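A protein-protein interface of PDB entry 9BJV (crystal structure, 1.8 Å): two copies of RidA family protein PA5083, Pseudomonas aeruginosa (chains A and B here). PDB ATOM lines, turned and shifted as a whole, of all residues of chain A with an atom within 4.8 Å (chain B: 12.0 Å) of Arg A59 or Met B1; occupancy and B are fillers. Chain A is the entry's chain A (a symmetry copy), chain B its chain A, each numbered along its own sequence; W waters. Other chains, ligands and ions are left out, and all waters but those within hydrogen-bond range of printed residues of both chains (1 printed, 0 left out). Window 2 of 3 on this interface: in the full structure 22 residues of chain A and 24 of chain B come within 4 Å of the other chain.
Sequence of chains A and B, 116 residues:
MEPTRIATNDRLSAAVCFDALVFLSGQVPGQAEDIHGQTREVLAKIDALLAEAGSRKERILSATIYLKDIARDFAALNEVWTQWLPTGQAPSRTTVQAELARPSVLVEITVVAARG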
ATOM      1  N   SER A  55      -0.401   8.458  -2.730  1.00  0.00           N
ATOM      2  CA  SER A  55      -0.327   9.904  -2.903  1.00  0.00           C
ATOM      3  C   SER A  55      -0.317  10.239  -4.394  1.00  0.00           C
ATOM      4  O   SER A  55      -0.713   9.416  -5.230  1.00  0.00           O
ATOM      5  CB  SER A  55       0.928  10.466  -2.202  1.00  0.00           C
ATOM      6  OG  SER A  55       0.900  11.890  -2.125  1.00  0.00           O
ATOM      7  N   ARG A  56       0.154  11.433  -4.730  1.00  0.00           N
ATOM      8  CA  ARG A  56       0.197  11.926  -6.102  1.00  0.00           C
ATOM      9  C   ARG A  56       0.984  13.231  -6.098  1.00  0.00           C
ATOM     10  O   ARG A  56       1.268  13.800  -5.041  1.00  0.00           O
ATOM     11  CB  ARG A  56      -1.209  12.134  -6.681  1.00  0.00           C
ATOM     12  CG  ARG A  56      -2.087  13.077  -5.864  1.00  0.00           C
ATOM     13  CD  ARG A  56      -3.526  13.141  -6.400  1.00  0.00           C
ATOM     14  NE  ARG A  56      -3.604  13.738  -7.732  1.00  0.00           N
ATOM     15  CZ  ARG A  56      -4.721  13.843  -8.449  1.00  0.00           C
ATOM     16  NH1 ARG A  56      -5.885  13.414  -7.987  1.00  0.00           N
ATOM     17  NH2 ARG A  56      -4.666  14.391  -9.659  1.00  0.00           N
ATOM     18  N   LYS A  57       1.319  13.705  -7.302  1.00  0.00           N
ATOM     19  CA  LYS A  57       2.205  14.861  -7.419  1.00  0.00           C
ATOM     20  C   LYS A  57       1.596  16.097  -6.772  1.00  0.00           C
ATOM     21  O   LYS A  57       2.309  16.903  -6.156  1.00  0.00           O
ATOM     22  CB  LYS A  57       2.521  15.135  -8.889  1.00  0.00           C
ATOM     23  CG  LYS A  57       3.307  14.040  -9.565  1.00  0.00           C
ATOM     24  CD  LYS A  57       3.971  14.586 -10.833  1.00  0.00           C
ATOM     25  CE  LYS A  57       3.157  14.325 -12.078  1.00  0.00           C
ATOM     26  NZ  LYS A  57       3.864  14.837 -13.295  1.00  0.00           N
ATOM     27  N   GLU A  58       0.277  16.256  -6.890  1.00  0.00           N
ATOM     28  CA  GLU A  58      -0.411  17.398  -6.306  1.00  0.00           C
ATOM     29  C   GLU A  58      -0.365  17.413  -4.781  1.00  0.00           C
ATOM     30  O   GLU A  58      -0.785  18.406  -4.174  1.00  0.00           O
ATOM     31  CB  GLU A  58      -1.874  17.409  -6.769  1.00  0.00           C
ATOM     32  CG  GLU A  58      -2.068  17.614  -8.268  1.00  0.00           C
ATOM     33  CD  GLU A  58      -1.931  16.336  -9.098  1.00  0.00           C
ATOM     34  OE1 GLU A  58      -1.519  15.279  -8.567  1.00  0.00           O
ATOM     35  OE2 GLU A  58      -2.242  16.399 -10.307  1.00  0.00           O
ATOM     36  N   ARG A  59       0.100  16.340  -4.144  1.00  0.00           N
ATOM     37  CA  ARG A  59       0.065  16.251  -2.689  1.00  0.00           C
ATOM     38  C   ARG A  59       1.463  16.178  -2.081  1.00  0.00           C
ATOM     39  O   ARG A  59       1.610  15.829  -0.907  1.00  0.00           O
ATOM     40  CB  ARG A  59      -0.790  15.066  -2.256  1.00  0.00           C
ATOM     41  CG  ARG A  59      -2.254  15.295  -2.656  1.00  0.00           C
ATOM     42  CD  ARG A  59      -3.144  14.131  -2.312  1.00  0.00           C
ATOM     43  NE  ARG A  59      -3.323  14.006  -0.872  1.00  0.00           N
ATOM     44  CZ  ARG A  59      -4.282  14.604  -0.173  1.00  0.00           C
ATOM     45  NH1 ARG A  59      -5.160  15.410  -0.750  1.00  0.00           N
ATOM     46  NH2 ARG A  59      -4.363  14.379   1.137  1.00  0.00           N
ATOM     47  N   ILE A  60       2.489  16.531  -2.853  1.00  0.00           N
ATOM     48  CA  ILE A  60       3.830  16.670  -2.295  1.00  0.00           C
ATOM     49  C   ILE A  60       3.853  17.835  -1.313  1.00  0.00           C
ATOM     50  O   ILE A  60       3.321  18.921  -1.587  1.00  0.00           O
ATOM     51  CB  ILE A  60       4.856  16.858  -3.426  1.00  0.00           C
ATOM     52  CG1 ILE A  60       4.811  15.665  -4.392  1.00  0.00           C
ATOM     53  CG2 ILE A  60       6.274  17.010  -2.858  1.00  0.00           C
ATOM     54  CD1 ILE A  60       5.577  15.893  -5.706  1.00  0.00           C
ATOM     55  N   LEU A  61       4.474  17.613  -0.159  1.00  0.00           N
ATOM     56  CA  LEU A  61       4.608  18.641   0.866  1.00  0.00           C
ATOM     57  C   LEU A  61       5.980  19.311   0.845  1.00  0.00           C
ATOM     58  O   LEU A  61       6.070  20.539   0.998  1.00  0.00           O
ATOM     59  CB  LEU A  61       4.349  18.033   2.253  1.00  0.00           C
ATOM     60  CG  LEU A  61       3.012  17.282   2.378  1.00  0.00           C
ATOM     61  CD1 LEU A  61       2.952  16.459   3.668  1.00  0.00           C
ATOM     62  CD2 LEU A  61       1.845  18.262   2.294  1.00  0.00           C
ATOM     63  N   ALA A 113       5.248  13.634   1.281  1.00  0.00           N
ATOM     64  CA  ALA A 113       3.969  13.899   0.623  1.00  0.00           C
ATOM     65  C   ALA A 113       2.806  13.485   1.524  1.00  0.00           C
ATOM     66  O   ALA A 113       2.977  12.787   2.525  1.00  0.00           O
ATOM     67  CB  ALA A 113       3.877  13.159  -0.713  1.00  0.00           C
ATOM     68  N   ALA A 114       1.603  13.917   1.147  1.00  0.00           N
ATOM     69  CA  ALA A 114       0.393  13.622   1.908  1.00  0.00           C
ATOM     70  C   ALA A 114      -0.354  12.476   1.243  1.00  0.00           C
ATOM     71  O   ALA A 114      -0.531  12.467   0.021  1.00  0.00           O
ATOM     72  CB  ALA A 114      -0.513  14.851   2.001  1.00  0.00           C
ATOM     73  N   ARG A 115      -0.780  11.508   2.044  1.00  0.00           N
ATOM     74  CA  ARG A 115      -1.602  10.434   1.502  1.00  0.00           C
ATOM     75  C   ARG A 115      -2.990  10.974   1.201  1.00  0.00           C
ATOM     76  O   ARG A 115      -3.564  11.718   2.004  1.00  0.00           O
ATOM     77  CB  ARG A 115      -1.672   9.257   2.476  1.00  0.00           C
ATOM     78  CG  ARG A 115      -0.845   8.075   2.006  1.00  0.00           C
ATOM     79  CD  ARG A 115      -0.840   6.915   2.990  1.00  0.00           C
ATOM     80  NE  ARG A 115      -2.088   6.166   2.923  1.00  0.00           N
ATOM     81  CZ  ARG A 115      -2.225   4.986   2.333  1.00  0.00           C
ATOM     82  NH1 ARG A 115      -1.190   4.353   1.799  1.00  0.00           N
ATOM     83  NH2 ARG A 115      -3.428   4.420   2.289  1.00  0.00           N
ATOM     84  N   GLY A 116      -3.508  10.626   0.028  1.00  0.00           N
ATOM     85  CA  GLY A 116      -4.786  11.124  -0.440  1.00  0.00           C
ATOM     86  C   GLY A 116      -4.782  11.238  -1.953  1.00  0.00           C
ATOM     87  O   GLY A 116      -3.774  10.929  -2.597  1.00  0.00           O
ATOM     88  N   MET B   1      -8.855  15.968   3.302  1.00  0.00           N
ATOM     89  CA  MET B   1      -7.893  17.003   3.672  1.00  0.00           C
ATOM     90  C   MET B   1      -6.832  17.169   2.592  1.00  0.00           C
ATOM     91  O   MET B   1      -6.100  16.228   2.282  1.00  0.00           O
ATOM     92  CB  MET B   1      -7.235  16.663   5.006  1.00  0.00           C
ATOM     93  CG  MET B   1      -6.214  17.681   5.478  1.00  0.00           C
ATOM     94  SD  MET B   1      -5.643  17.292   7.145  1.00  0.00           S
ATOM     95  CE  MET B   1      -7.174  17.418   8.065  1.00  0.00           C
ATOM     96  N   GLU B   2      -6.756  18.362   2.007  1.00  0.00           N
ATOM     97  CA  GLU B   2      -5.765  18.610   0.977  1.00  0.00           C
ATOM     98  C   GLU B   2      -4.767  19.661   1.447  1.00  0.00           C
ATOM     99  O   GLU B   2      -5.100  20.509   2.282  1.00  0.00           O
ATOM    100  CB  GLU B   2      -6.420  19.072  -0.331  1.00  0.00           C
ATOM    101  CG  GLU B   2      -7.238  17.987  -1.020  1.00  0.00           C
ATOM    102  CD  GLU B   2      -7.659  18.377  -2.421  1.00  0.00           C
ATOM    103  OE1 GLU B   2      -7.493  19.562  -2.786  1.00  0.00           O
ATOM    104  OE2 GLU B   2      -8.153  17.497  -3.161  1.00  0.00           O
ATOM    105  N   PRO B   3      -3.529  19.609   0.957  1.00  0.00           N
ATOM    106  CA  PRO B   3      -2.547  20.633   1.337  1.00  0.00           C
ATOM    107  C   PRO B   3      -2.990  22.015   0.877  1.00  0.00           C
ATOM    108  O   PRO B   3      -3.631  22.171  -0.164  1.00  0.00           O
ATOM    109  CB  PRO B   3      -1.270  20.192   0.611  1.00  0.00           C
ATOM    110  CG  PRO B   3      -1.449  18.733   0.370  1.00  0.00           C
ATOM    111  CD  PRO B   3      -2.927  18.529   0.156  1.00  0.00           C
ATOM    112  N   THR B   4      -2.647  23.028   1.667  1.00  0.00           N
ATOM    113  CA  THR B   4      -2.785  24.411   1.230  1.00  0.00           C
ATOM    114  C   THR B   4      -1.405  25.040   1.105  1.00  0.00           C
ATOM    115  O   THR B   4      -0.427  24.568   1.693  1.00  0.00           O
ATOM    116  CB  THR B   4      -3.666  25.223   2.184  1.00  0.00           C
ATOM    117  OG1 THR B   4      -3.166  25.108   3.519  1.00  0.00           O
ATOM    118  CG2 THR B   4      -5.104  24.721   2.132  1.00  0.00           C
ATOM    119  N   ARG B   5      -1.322  26.097   0.304  1.00  0.00           N
ATOM    120  CA  ARG B   5      -0.033  26.651  -0.081  1.00  0.00           C
ATOM    121  C   ARG B   5      -0.023  28.162   0.075  1.00  0.00           C
ATOM    122  O   ARG B   5      -1.059  28.825  -0.010  1.00  0.00           O
ATOM    123  CB  ARG B   5       0.321  26.284  -1.525  1.00  0.00           C
ATOM    124  CG  ARG B   5       0.257  24.796  -1.801  1.00  0.00           C
ATOM    125  CD  ARG B   5       0.558  24.487  -3.246  1.00  0.00           C
ATOM    126  NE  ARG B   5       0.556  23.047  -3.462  1.00  0.00           N
ATOM    127  CZ  ARG B   5      -0.537  22.330  -3.668  1.00  0.00           C
ATOM    128  NH1 ARG B   5      -1.730  22.901  -3.749  1.00  0.00           N
ATOM    129  NH2 ARG B   5      -0.432  21.010  -3.788  1.00  0.00           N
ATOM    130  N   THR B   8       2.946  30.653  -4.092  1.00  0.00           N
ATOM    131  CA  THR B   8       3.236  29.615  -5.070  1.00  0.00           C
ATOM    132  C   THR B   8       3.746  30.234  -6.367  1.00  0.00           C
ATOM    133  O   THR B   8       3.124  31.158  -6.906  1.00  0.00           O
ATOM    134  CB  THR B   8       1.979  28.786  -5.353  1.00  0.00           C
ATOM    135  OG1 THR B   8       1.498  28.216  -4.132  1.00  0.00           O
ATOM    136  CG2 THR B   8       2.275  27.676  -6.363  1.00  0.00           C
ATOM    137  N   SER B  13       6.357  26.536  -3.529  1.00  0.00           N
ATOM    138  CA  SER B  13       5.560  27.370  -2.649  1.00  0.00           C
ATOM    139  C   SER B  13       6.381  27.677  -1.403  1.00  0.00           C
ATOM    140  O   SER B  13       7.039  26.789  -0.848  1.00  0.00           O
ATOM    141  CB  SER B  13       4.246  26.688  -2.240  1.00  0.00           C
ATOM    142  OG  SER B  13       3.435  26.385  -3.365  1.00  0.00           O
ATOM    143  N   ALA B  15       5.384  28.097   1.512  1.00  0.00           N
ATOM    144  CA  ALA B  15       4.887  27.262   2.598  1.00  0.00           C
ATOM    145  C   ALA B  15       3.797  26.340   2.075  1.00  0.00           C
ATOM    146  O   ALA B  15       2.995  26.733   1.220  1.00  0.00           O
ATOM    147  CB  ALA B  15       4.320  28.090   3.751  1.00  0.00           C
ATOM    148  N   VAL B  16       3.771  25.122   2.606  1.00  0.00           N
ATOM    149  CA  VAL B  16       2.708  24.164   2.345  1.00  0.00           C
ATOM    150  C   VAL B  16       2.218  23.655   3.687  1.00  0.00           C
ATOM    151  O   VAL B  16       3.020  23.203   4.508  1.00  0.00           O
ATOM    152  CB  VAL B  16       3.185  22.997   1.463  1.00  0.00           C
ATOM    153  CG1 VAL B  16       2.081  21.951   1.339  1.00  0.00           C
ATOM    154  CG2 VAL B  16       3.611  23.506   0.085  1.00  0.00           C
ATOM    155  N   CYS B  17       0.913  23.743   3.917  1.00  0.00           N
ATOM    156  CA  CYS B  17       0.303  23.280   5.154  1.00  0.00           C
ATOM    157  C   CYS B  17      -0.513  22.021   4.906  1.00  0.00           C
ATOM    158  O   CYS B  17      -1.207  21.904   3.893  1.00  0.00           O
ATOM    159  CB  CYS B  17      -0.587  24.367   5.763  1.00  0.00           C
ATOM    160  SG  CYS B  17       0.322  25.914   6.065  1.00  0.00           S
ATOM    161  N   PHE B  18      -0.446  21.088   5.848  1.00  0.00           N
ATOM    162  CA  PHE B  18      -1.231  19.867   5.756  1.00  0.00           C
ATOM    163  C   PHE B  18      -1.427  19.356   7.163  1.00  0.00           C
ATOM    164  O   PHE B  18      -0.445  19.189   7.891  1.00  0.00           O
ATOM    165  CB  PHE B  18      -0.535  18.803   4.907  1.00  0.00           C
ATOM    166  CG  PHE B  18      -1.273  17.501   4.856  1.00  0.00           C
ATOM    167  CD1 PHE B  18      -2.496  17.412   4.204  1.00  0.00           C
ATOM    168  CD2 PHE B  18      -0.755  16.373   5.461  1.00  0.00           C
ATOM    169  CE1 PHE B  18      -3.188  16.205   4.159  1.00  0.00           C
ATOM    170  CE2 PHE B  18      -1.447  15.163   5.423  1.00  0.00           C
ATOM    171  CZ  PHE B  18      -2.660  15.085   4.773  1.00  0.00           C
ATOM    172  N   ASP B  19      -2.676  19.095   7.534  1.00  0.00           N
ATOM    173  CA  ASP B  19      -2.984  18.634   8.887  1.00  0.00           C
ATOM    174  C   ASP B  19      -2.540  19.779   9.797  1.00  0.00           C
ATOM    175  O   ASP B  19      -2.860  20.944   9.515  1.00  0.00           O
ATOM    176  CB  ASP B  19      -2.311  17.286   9.135  1.00  0.00           C
ATOM    177  CG  ASP B  19      -3.193  16.312   9.885  1.00  0.00           C
ATOM    178  OD1 ASP B  19      -2.871  15.101   9.871  1.00  0.00           O
ATOM    179  OD2 ASP B  19      -4.208  16.750  10.470  1.00  0.00           O
ATOM    180  N   ALA B  20      -1.779  19.514  10.848  1.00  0.00           N
ATOM    181  CA  ALA B  20      -1.278  20.571  11.714  1.00  0.00           C
ATOM    182  C   ALA B  20       0.188  20.875  11.449  1.00  0.00           C
ATOM    183  O   ALA B  20       0.873  21.408  12.329  1.00  0.00           O
ATOM    184  CB  ALA B  20      -1.491  20.190  13.177  1.00  0.00           C
ATOM    185  N   LEU B  21       0.684  20.544  10.256  1.00  0.00           N
ATOM    186  CA  LEU B  21       2.088  20.712   9.914  1.00  0.00           C
ATOM    187  C   LEU B  21       2.265  21.829   8.895  1.00  0.00           C
ATOM    188  O   LEU B  21       1.425  22.027   8.008  1.00  0.00           O
ATOM    189  CB  LEU B  21       2.683  19.412   9.344  1.00  0.00           C
ATOM    190  CG  LEU B  21       2.699  18.222  10.297  1.00  0.00           C
ATOM    191  CD1 LEU B  21       3.247  16.975   9.593  1.00  0.00           C
ATOM    192  CD2 LEU B  21       3.511  18.538  11.525  1.00  0.00           C
ATOM    193  N   VAL B  22       3.382  22.546   9.033  1.00  0.00           N
ATOM    194  CA  VAL B  22       3.779  23.614   8.122  1.00  0.00           C
ATOM    195  C   VAL B  22       5.162  23.270   7.582  1.00  0.00           C
ATOM    196  O   VAL B  22       6.112  23.130   8.362  1.00  0.00           O
ATOM    197  CB  VAL B  22       3.803  24.981   8.835  1.00  0.00           C
ATOM    198  CG1 VAL B  22       4.300  26.059   7.900  1.00  0.00           C
ATOM    199  CG2 VAL B  22       2.416  25.320   9.376  1.00  0.00           C
ATOM    200  N   PHE B  23       5.281  23.147   6.258  1.00  0.00           N
ATOM    201  CA  PHE B  23       6.555  22.876   5.591  1.00  0.00           C
ATOM    202  C   PHE B  23       6.997  24.130   4.846  1.00  0.00           C
ATOM    203  O   PHE B  23       6.320  24.557   3.908  1.00  0.00           O
ATOM    204  CB  PHE B  23       6.428  21.717   4.601  1.00  0.00           C
ATOM    205  CG  PHE B  23       5.980  20.426   5.234  1.00  0.00           C
ATOM    206  CD1 PHE B  23       4.638  20.207   5.523  1.00  0.00           C
ATOM    207  CD2 PHE B  23       6.902  19.435   5.531  1.00  0.00           C
ATOM    208  CE1 PHE B  23       4.217  19.015   6.114  1.00  0.00           C
ATOM    209  CE2 PHE B  23       6.493  18.241   6.125  1.00  0.00           C
ATOM    210  CZ  PHE B  23       5.144  18.032   6.411  1.00  0.00           C
ATOM    211  N   ARG B 115       1.273  23.874  13.182  1.00  0.00           N
ATOM    212  CA  ARG B 115       0.243  24.903  13.133  1.00  0.00           C
ATOM    213  C   ARG B 115      -0.400  25.027  14.503  1.00  0.00           C
ATOM    214  O   ARG B 115      -0.698  24.020  15.154  1.00  0.00           O
ATOM    215  CB  ARG B 115      -0.803  24.577  12.066  1.00  0.00           C
ATOM    216  CG  ARG B 115      -0.673  25.469  10.846  1.00  0.00           C
ATOM    217  CD  ARG B 115      -1.656  25.121   9.739  1.00  0.00           C
ATOM    218  NE  ARG B 115      -2.991  25.613  10.051  1.00  0.00           N
ATOM    219  CZ  ARG B 115      -3.548  26.681   9.496  1.00  0.00           C
ATOM    220  NH1 ARG B 115      -2.933  27.366   8.542  1.00  0.00           N
ATOM    221  NH2 ARG B 115      -4.755  27.066   9.900  1.00  0.00           N
HETATM  222  O   HOH W   1       2.110  20.738  -3.231  1.00  0.00           O
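The guanidinium group (NH2) of Arg B5 sits at hydrogen-bond distance from the backbone carbonyl oxygen (O) of Glu A58, 2.7 Å away. NH2 of Arg A59 is in hydrogen-bond range of O of Met B1 (2.8 Å).
O of Val B16 sits at hydrogen-bond distance from N of Phe B23, at 2.9 Å. N of Ala A114 sits at hydrogen-bond distance from O of Arg A59 (2.8 Å). The backbone carbonyl oxygen of Arg A115 sits at hydrogen-bond distance from the guanidinium group of Arg A59. SD of Met B1 sits close to N of Asp B19 (3.5 Å). The guanidinium group of Arg A56 lies within salt-bridge range of the side-chain carboxylate of Glu A58, 2.7 Å away. O of Ala A114 is in hydrogen-bond range of OG of Ser A55, at 2.6 Å.
Arg A59 touches Glu B2. Arg A59 touches Pro B3 (NH1 to CD, 3.9 Å). CE1 of Phe B18 touches NH2 of Arg A59 (3.7 Å). CG of Pro B3 touches CD2 of Leu A61 (3.8 Å). CD2 of Leu A61 touches CG1 of Val B16 (3.8 Å). CB of Phe B18 touches CD2 of Leu A61, at 3.6 Å. CE1 of Phe B23 touches CD1 of Leu A61, 3.8 Å away. Phe B18 touches Ala A114.
Arg A59 touches just these residues of chain B: Met B1, Glu B2, Pro B3 and Phe B18. Met B1 touches just one residue of chain A: Arg A59 (2.8 Å). No residue of chain B comes within 4 Å of Ser A55. Glu A58 touches just one residue of chain B: Arg B5. No residue of chain B comes within 4 Å of Ala A113. Of the printed residues of chain B, Ala A114 touches Phe B18. No residue of chain B comes within 4 Å of Gly A116. Printed residues of chain A within 4 Å of Pro B3: Arg A59 (3.9 Å) and Leu A61 (3.8 Å). Of the printed residues of chain A, Glu B2 touches Arg A59. Of the printed residues of chain A, Phe B18 touches Arg A59 (3.7 Å), Leu A61 (3.6 Å) and Ala A114 (3.5 Å). Of the printed residues of chain A, Val B16 touches Leu A61 (3.8 Å). Val B22 touches none of the printed residues of chain A. Lys A57 touches none of the printed residues of chain B. The nearest residue of chain B that does not touch Arg A59 is Arg B5 (4.7 Å). The nearest printed residue of chain A that does not touch Met B1 is Arg A115 (5.2 Å).
Hydrophobic or aromatic side chains of chain A that line the printed part of chain B: Leu A61 and Ala A114. Of the 17 printed residues of chain B, 7 touch a printed residue of chain A. Hydrophobic or aromatic side chains of chain B within 4 Å of the printed part of chain A: Pro B3, Val B16, Phe B18 and Phe B23. Among the printed residues, no Asp or Glu carboxylate lies within 4 Å of a Lys or Arg side-chain nitrogen of the other chain.
Position printed for both chains: 115. Of the 10 pairs that touch across the chains among the printed residues, none has its exchanged pair printed and touching as well.
Water W1 lies within hydrogen-bond range of NH2 of Arg B5 (2.6 Å) and O of Ile A60 (2.7 Å).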
